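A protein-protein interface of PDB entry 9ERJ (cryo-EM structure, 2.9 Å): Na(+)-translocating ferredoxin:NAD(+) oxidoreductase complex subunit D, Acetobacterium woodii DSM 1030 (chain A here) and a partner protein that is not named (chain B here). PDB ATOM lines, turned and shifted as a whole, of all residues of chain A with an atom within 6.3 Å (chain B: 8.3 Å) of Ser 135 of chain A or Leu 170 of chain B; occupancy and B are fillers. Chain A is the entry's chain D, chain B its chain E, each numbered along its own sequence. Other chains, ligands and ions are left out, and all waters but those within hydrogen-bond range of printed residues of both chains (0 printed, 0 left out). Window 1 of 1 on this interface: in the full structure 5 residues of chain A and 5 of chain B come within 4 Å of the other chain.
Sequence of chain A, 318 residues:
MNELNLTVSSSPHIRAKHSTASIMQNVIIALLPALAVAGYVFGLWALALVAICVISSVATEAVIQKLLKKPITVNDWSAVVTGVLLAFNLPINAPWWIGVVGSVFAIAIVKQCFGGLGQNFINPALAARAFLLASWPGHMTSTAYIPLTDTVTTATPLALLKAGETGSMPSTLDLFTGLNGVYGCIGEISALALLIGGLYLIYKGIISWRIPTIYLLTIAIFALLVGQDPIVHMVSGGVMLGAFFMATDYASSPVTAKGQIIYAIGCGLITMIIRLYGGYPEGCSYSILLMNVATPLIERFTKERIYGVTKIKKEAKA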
ATOM      1  N   ALA A 130     -16.212  -5.153   7.646  1.00  0.00           N
ATOM      2  CA  ALA A 130     -16.211  -4.917   6.206  1.00  0.00           C
ATOM      3  C   ALA A 130     -14.952  -4.202   5.737  1.00  0.00           C
ATOM      4  O   ALA A 130     -14.466  -4.489   4.637  1.00  0.00           O
ATOM      5  CB  ALA A 130     -17.446  -4.113   5.804  1.00  0.00           C
ATOM      6  N   PHE A 131     -14.423  -3.274   6.536  1.00  0.00           N
ATOM      7  CA  PHE A 131     -13.154  -2.633   6.210  1.00  0.00           C
ATOM      8  C   PHE A 131     -11.988  -3.613   6.268  1.00  0.00           C
ATOM      9  O   PHE A 131     -11.127  -3.601   5.379  1.00  0.00           O
ATOM     10  CB  PHE A 131     -12.932  -1.444   7.153  1.00  0.00           C
ATOM     11  CG  PHE A 131     -11.489  -1.150   7.461  1.00  0.00           C
ATOM     12  CD1 PHE A 131     -10.703  -0.441   6.568  1.00  0.00           C
ATOM     13  CD2 PHE A 131     -10.931  -1.542   8.669  1.00  0.00           C
ATOM     14  CE1 PHE A 131      -9.382  -0.159   6.858  1.00  0.00           C
ATOM     15  CE2 PHE A 131      -9.611  -1.262   8.963  1.00  0.00           C
ATOM     16  CZ  PHE A 131      -8.837  -0.569   8.057  1.00  0.00           C
ATOM     17  N   LEU A 132     -11.952  -4.476   7.289  1.00  0.00           N
ATOM     18  CA  LEU A 132     -10.883  -5.466   7.406  1.00  0.00           C
ATOM     19  C   LEU A 132     -10.919  -6.485   6.274  1.00  0.00           C
ATOM     20  O   LEU A 132      -9.866  -6.890   5.772  1.00  0.00           O
ATOM     21  CB  LEU A 132     -10.968  -6.184   8.753  1.00  0.00           C
ATOM     22  CG  LEU A 132     -10.603  -5.405  10.015  1.00  0.00           C
ATOM     23  CD1 LEU A 132     -10.972  -6.207  11.247  1.00  0.00           C
ATOM     24  CD2 LEU A 132      -9.126  -5.062  10.022  1.00  0.00           C
ATOM     25  N   LEU A 133     -12.115  -6.927   5.874  1.00  0.00           N
ATOM     26  CA  LEU A 133     -12.219  -7.924   4.813  1.00  0.00           C
ATOM     27  C   LEU A 133     -11.755  -7.364   3.473  1.00  0.00           C
ATOM     28  O   LEU A 133     -11.127  -8.075   2.681  1.00  0.00           O
ATOM     29  CB  LEU A 133     -13.656  -8.440   4.716  1.00  0.00           C
ATOM     30  CG  LEU A 133     -14.028  -9.314   3.517  1.00  0.00           C
ATOM     31  CD1 LEU A 133     -13.257 -10.621   3.538  1.00  0.00           C
ATOM     32  CD2 LEU A 133     -15.523  -9.579   3.488  1.00  0.00           C
ATOM     33  N   ALA A 134     -12.055  -6.094   3.201  1.00  0.00           N
ATOM     34  CA  ALA A 134     -11.635  -5.485   1.944  1.00  0.00           C
ATOM     35  C   ALA A 134     -10.153  -5.132   1.950  1.00  0.00           C
ATOM     36  O   ALA A 134      -9.484  -5.246   0.917  1.00  0.00           O
ATOM     37  CB  ALA A 134     -12.476  -4.242   1.657  1.00  0.00           C
ATOM     38  N   SER A 135      -9.620  -4.695   3.095  1.00  0.00           N
ATOM     39  CA  SER A 135      -8.226  -4.267   3.139  1.00  0.00           C
ATOM     40  C   SER A 135      -7.257  -5.444   3.095  1.00  0.00           C
ATOM     41  O   SER A 135      -6.247  -5.389   2.385  1.00  0.00           O
ATOM     42  CB  SER A 135      -7.980  -3.419   4.385  1.00  0.00           C
ATOM     43  OG  SER A 135      -8.943  -2.388   4.495  1.00  0.00           O
ATOM     44  N   TRP A 136      -7.538  -6.514   3.840  1.00  0.00           N
ATOM     45  CA  TRP A 136      -6.660  -7.684   3.920  1.00  0.00           C
ATOM     46  C   TRP A 136      -7.474  -8.933   3.611  1.00  0.00           C
ATOM     47  O   TRP A 136      -7.883  -9.663   4.523  1.00  0.00           O
ATOM     48  CB  TRP A 136      -5.997  -7.793   5.295  1.00  0.00           C
ATOM     49  CG  TRP A 136      -4.983  -6.724   5.564  1.00  0.00           C
ATOM     50  CD1 TRP A 136      -3.693  -6.692   5.126  1.00  0.00           C
ATOM     51  CD2 TRP A 136      -5.173  -5.535   6.340  1.00  0.00           C
ATOM     52  NE1 TRP A 136      -3.069  -5.554   5.575  1.00  0.00           N
ATOM     53  CE2 TRP A 136      -3.957  -4.828   6.323  1.00  0.00           C
ATOM     54  CE3 TRP A 136      -6.255  -5.000   7.045  1.00  0.00           C
ATOM     55  CZ2 TRP A 136      -3.793  -3.614   6.982  1.00  0.00           C
ATOM     56  CZ3 TRP A 136      -6.090  -3.796   7.697  1.00  0.00           C
ATOM     57  CH2 TRP A 136      -4.868  -3.116   7.662  1.00  0.00           C
ATOM     58  N   PRO A 137      -7.730  -9.210   2.329  1.00  0.00           N
ATOM     59  CA  PRO A 137      -8.569 -10.371   1.995  1.00  0.00           C
ATOM     60  C   PRO A 137      -7.872 -11.706   2.187  1.00  0.00           C
ATOM     61  O   PRO A 137      -8.551 -12.735   2.271  1.00  0.00           O
ATOM     62  CB  PRO A 137      -8.925 -10.129   0.523  1.00  0.00           C
ATOM     63  CG  PRO A 137      -7.788  -9.330  -0.002  1.00  0.00           C
ATOM     64  CD  PRO A 137      -7.306  -8.467   1.130  1.00  0.00           C
ATOM     65  N   LEU B 151      -0.025   5.183   2.043  1.00  0.00           N
ATOM     66  CA  LEU B 151      -0.715   4.142   2.797  1.00  0.00           C
ATOM     67  C   LEU B 151      -1.142   2.972   1.914  1.00  0.00           C
ATOM     68  O   LEU B 151      -0.994   1.813   2.314  1.00  0.00           O
ATOM     69  CB  LEU B 151      -1.925   4.727   3.525  1.00  0.00           C
ATOM     70  CG  LEU B 151      -1.641   5.353   4.893  1.00  0.00           C
ATOM     71  CD1 LEU B 151      -2.935   5.689   5.609  1.00  0.00           C
ATOM     72  CD2 LEU B 151      -0.786   4.429   5.745  1.00  0.00           C
ATOM     73  N   GLY B 152      -1.668   3.242   0.717  1.00  0.00           N
ATOM     74  CA  GLY B 152      -2.245   2.176  -0.082  1.00  0.00           C
ATOM     75  C   GLY B 152      -1.286   1.398  -0.956  1.00  0.00           C
ATOM     76  O   GLY B 152      -1.690   0.377  -1.520  1.00  0.00           O
ATOM     77  N   ALA B 153      -0.037   1.842  -1.093  1.00  0.00           N
ATOM     78  CA  ALA B 153       0.913   1.123  -1.934  1.00  0.00           C
ATOM     79  C   ALA B 153       2.250   0.941  -1.230  1.00  0.00           C
ATOM     80  O   ALA B 153       3.036   0.063  -1.598  1.00  0.00           O
ATOM     81  CB  ALA B 153       1.110   1.854  -3.263  1.00  0.00           C
ATOM     82  N   TYR B 166       5.801  -5.570   2.905  1.00  0.00           N
ATOM     83  CA  TYR B 166       4.691  -4.770   3.404  1.00  0.00           C
ATOM     84  C   TYR B 166       3.380  -5.207   2.760  1.00  0.00           C
ATOM     85  O   TYR B 166       3.317  -5.467   1.555  1.00  0.00           O
ATOM     86  CB  TYR B 166       4.956  -3.290   3.126  1.00  0.00           C
ATOM     87  CG  TYR B 166       3.856  -2.349   3.558  1.00  0.00           C
ATOM     88  CD1 TYR B 166       3.489  -2.239   4.891  1.00  0.00           C
ATOM     89  CD2 TYR B 166       3.199  -1.552   2.631  1.00  0.00           C
ATOM     90  CE1 TYR B 166       2.489  -1.373   5.287  1.00  0.00           C
ATOM     91  CE2 TYR B 166       2.199  -0.683   3.018  1.00  0.00           C
ATOM     92  CZ  TYR B 166       1.849  -0.598   4.346  1.00  0.00           C
ATOM     93  OH  TYR B 166       0.853   0.267   4.733  1.00  0.00           O
ATOM     94  N   GLU B 167       2.332  -5.293   3.575  1.00  0.00           N
ATOM     95  CA  GLU B 167       0.996  -5.620   3.088  1.00  0.00           C
ATOM     96  C   GLU B 167       0.130  -4.371   3.143  1.00  0.00           C
ATOM     97  O   GLU B 167      -0.246  -3.933   4.243  1.00  0.00           O
ATOM     98  CB  GLU B 167       0.374  -6.742   3.919  1.00  0.00           C
ATOM     99  CG  GLU B 167       1.350  -7.842   4.290  1.00  0.00           C
ATOM    100  CD  GLU B 167       0.660  -9.076   4.831  1.00  0.00           C
ATOM    101  OE1 GLU B 167      -0.413  -9.433   4.306  1.00  0.00           O
ATOM    102  OE2 GLU B 167       1.193  -9.689   5.779  1.00  0.00           O
ATOM    103  N   PRO B 168      -0.215  -3.773   2.006  1.00  0.00           N
ATOM    104  CA  PRO B 168      -0.855  -2.455   2.025  1.00  0.00           C
ATOM    105  C   PRO B 168      -2.307  -2.515   2.471  1.00  0.00           C
ATOM    106  O   PRO B 168      -2.953  -3.564   2.473  1.00  0.00           O
ATOM    107  CB  PRO B 168      -0.752  -1.993   0.566  1.00  0.00           C
ATOM    108  CG  PRO B 168       0.265  -2.901  -0.067  1.00  0.00           C
ATOM    109  CD  PRO B 168       0.100  -4.202   0.637  1.00  0.00           C
ATOM    110  N   VAL B 169      -2.815  -1.346   2.860  1.00  0.00           N
ATOM    111  CA  VAL B 169      -4.234  -1.155   3.150  1.00  0.00           C
ATOM    112  C   VAL B 169      -4.926  -0.916   1.812  1.00  0.00           C
ATOM    113  O   VAL B 169      -4.935   0.203   1.298  1.00  0.00           O
ATOM    114  CB  VAL B 169      -4.467   0.004   4.121  1.00  0.00           C
ATOM    115  CG1 VAL B 169      -5.898  -0.004   4.627  1.00  0.00           C
ATOM    116  CG2 VAL B 169      -3.487  -0.066   5.280  1.00  0.00           C
ATOM    117  N   LEU B 170      -5.517  -1.966   1.242  1.00  0.00           N
ATOM    118  CA  LEU B 170      -6.065  -1.916  -0.106  1.00  0.00           C
ATOM    119  C   LEU B 170      -7.430  -1.240  -0.177  1.00  0.00           C
ATOM    120  O   LEU B 170      -8.109  -1.349  -1.203  1.00  0.00           O
ATOM    121  CB  LEU B 170      -6.152  -3.326  -0.696  1.00  0.00           C
ATOM    122  CG  LEU B 170      -4.826  -4.061  -0.894  1.00  0.00           C
ATOM    123  CD1 LEU B 170      -5.070  -5.526  -1.206  1.00  0.00           C
ATOM    124  CD2 LEU B 170      -4.011  -3.404  -1.992  1.00  0.00           C
ATOM    125  N   LEU B 171      -7.851  -0.553   0.884  1.00  0.00           N
ATOM    126  CA  LEU B 171      -9.065   0.248   0.832  1.00  0.00           C
ATOM    127  C   LEU B 171      -8.803   1.693   0.433  1.00  0.00           C
ATOM    128  O   LEU B 171      -9.711   2.349  -0.089  1.00  0.00           O
ATOM    129  CB  LEU B 171      -9.784   0.225   2.188  1.00  0.00           C
ATOM    130  CG  LEU B 171     -11.250   0.669   2.196  1.00  0.00           C
ATOM    131  CD1 LEU B 171     -12.173  -0.496   1.887  1.00  0.00           C
ATOM    132  CD2 LEU B 171     -11.619   1.314   3.522  1.00  0.00           C
ATOM    133  N   MET B 172      -7.583   2.194   0.640  1.00  0.00           N
ATOM    134  CA  MET B 172      -7.250   3.563   0.272  1.00  0.00           C
ATOM    135  C   MET B 172      -7.194   3.773  -1.233  1.00  0.00           C
ATOM    136  O   MET B 172      -7.300   4.915  -1.690  1.00  0.00           O
ATOM    137  CB  MET B 172      -5.913   3.961   0.897  1.00  0.00           C
ATOM    138  CG  MET B 172      -5.810   3.642   2.374  1.00  0.00           C
ATOM    139  SD  MET B 172      -6.525   4.942   3.390  1.00  0.00           S
ATOM    140  CE  MET B 172      -5.459   6.312   2.956  1.00  0.00           C
ATOM    141  N   ILE B 173      -7.032   2.706  -2.008  1.00  0.00           N
ATOM    142  CA  ILE B 173      -7.063   2.787  -3.459  1.00  0.00           C
ATOM    143  C   ILE B 173      -8.422   2.352  -4.010  1.00  0.00           C
ATOM    144  O   ILE B 173      -8.528   1.979  -5.177  1.00  0.00           O
ATOM    145  CB  ILE B 173      -5.919   1.979  -4.090  1.00  0.00           C
ATOM    146  CG1 ILE B 173      -6.007   0.513  -3.663  1.00  0.00           C
ATOM    147  CG2 ILE B 173      -4.576   2.572  -3.704  1.00  0.00           C
ATOM    148  CD1 ILE B 173      -4.923  -0.358  -4.248  1.00  0.00           C
ATOM    149  N   LEU B 174      -9.459   2.401  -3.186  1.00  0.00           N
ATOM    150  CA  LEU B 174     -10.822   2.037  -3.532  1.00  0.00           C
ATOM    151  C   LEU B 174     -11.712   3.270  -3.425  1.00  0.00           C
ATOM    152  O   LEU B 174     -11.322   4.269  -2.809  1.00  0.00           O
ATOM    153  CB  LEU B 174     -11.335   0.926  -2.602  1.00  0.00           C
ATOM    154  CG  LEU B 174     -10.853  -0.497  -2.902  1.00  0.00           C
ATOM    155  CD1 LEU B 174     -11.719  -1.521  -2.186  1.00  0.00           C
ATOM    156  CD2 LEU B 174     -10.825  -0.768  -4.398  1.00  0.00           C
ATOM    157  N   PRO B 175     -12.891   3.255  -4.048  1.00  0.00           N
ATOM    158  CA  PRO B 175     -13.799   4.418  -3.978  1.00  0.00           C
ATOM    159  C   PRO B 175     -14.152   4.842  -2.557  1.00  0.00           C
ATOM    160  O   PRO B 175     -14.218   6.054  -2.297  1.00  0.00           O
ATOM    161  CB  PRO B 175     -15.038   3.942  -4.753  1.00  0.00           C
ATOM    162  CG  PRO B 175     -14.488   3.003  -5.755  1.00  0.00           C
ATOM    163  CD  PRO B 175     -13.317   2.307  -5.099  1.00  0.00           C
ATOM    164  N   PRO B 176     -14.395   3.933  -1.602  1.00  0.00           N
ATOM    165  CA  PRO B 176     -14.673   4.408  -0.237  1.00  0.00           C
ATOM    166  C   PRO B 176     -13.461   4.939   0.511  1.00  0.00           C
ATOM    167  O   PRO B 176     -13.637   5.580   1.553  1.00  0.00           O
ATOM    168  CB  PRO B 176     -15.236   3.159   0.463  1.00  0.00           C
ATOM    169  CG  PRO B 176     -15.641   2.260  -0.617  1.00  0.00           C
ATOM    170  CD  PRO B 176     -14.626   2.476  -1.666  1.00  0.00           C
ATOM    171  N   GLY B 177     -12.246   4.702   0.026  1.00  0.00           N
ATOM    172  CA  GLY B 177     -11.061   5.141   0.737  1.00  0.00           C
ATOM    173  C   GLY B 177     -10.684   6.579   0.456  1.00  0.00           C
ATOM    174  O   GLY B 177      -9.814   7.142   1.125  1.00  0.00           O
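The backbone carbonyl oxygen of Phe 131 of chain A lies within hydrogen-bond range of the side-chain hydroxyl of Ser 135 of chain A (2.7 Å).
O of Leu 171 of chain B sits close to N of Gly 177 of chain B (3.5 Å).
Among the printed residues, merely in contact across the chains: Trp 136 of chain A with Glu 167 of chain B, Ser 135 of chain A with Leu 171 of chain B, Phe 131 of chain A with Leu 171 of chain B, Ser 135 of chain A with Leu 170 of chain B, Trp 136 of chain A with Pro 168 of chain B, Ala 134 of chain A with Leu 171 of chain B, Ser 135 of chain A with Pro 168 of chain B, Ser 135 of chain A with Val 169 of chain B and Trp 136 of chain A with Val 169 of chain B.
Printed residues of chain B within 4 Å of Ala 134 of chain A: Leu 171 (3.8 Å).
Ser 135 of chain A touches just these residues of chain B: Pro 168 (3.8 Å), Val 169 (3.9 Å), Leu 170 (3.7 Å) and Leu 171 (3.6 Å).
Printed residues of chain B within 4 Å of Trp 136 of chain A: Glu 167 (3.5 Å), Pro 168 (3.7 Å) and Val 169 (3.9 Å).
Printed residues of chain A within 4 Å of Glu 167 of chain B: Trp 136.
Printed residues of chain A within 4 Å of Pro 168 of chain B: Ser 135 (3.8 Å) and Trp 136 (3.7 Å).
Printed residues of chain A within 4 Å of Val 169 of chain B: Ser 135 and Trp 136.
Leu 170 of chain B touches just one residue of chain A: Ser 135.
Of the printed residues of chain A, Leu 171 of chain B touches Phe 131 (3.6 Å), Ala 134 (3.8 Å) and Ser 135 (3.6 Å).
The nearest residue of chain B that does not touch Ser 135 of chain A is Met 172 of chain B (6.1 Å).
The nearest residue of chain A that does not touch Leu 170 of chain B is Ala 134 of chain A (4.2 Å).
Along chain A the printed residues that touch a printed residue of chain B span positions 131 to 136.
Of the 15 printed residues of chain B, 5 touch a printed residue of chain A.
Along chain B the printed residues that touch a printed residue of chain A span positions 167 to 171.
Among the printed residues, 9 pairs touch across the chains.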
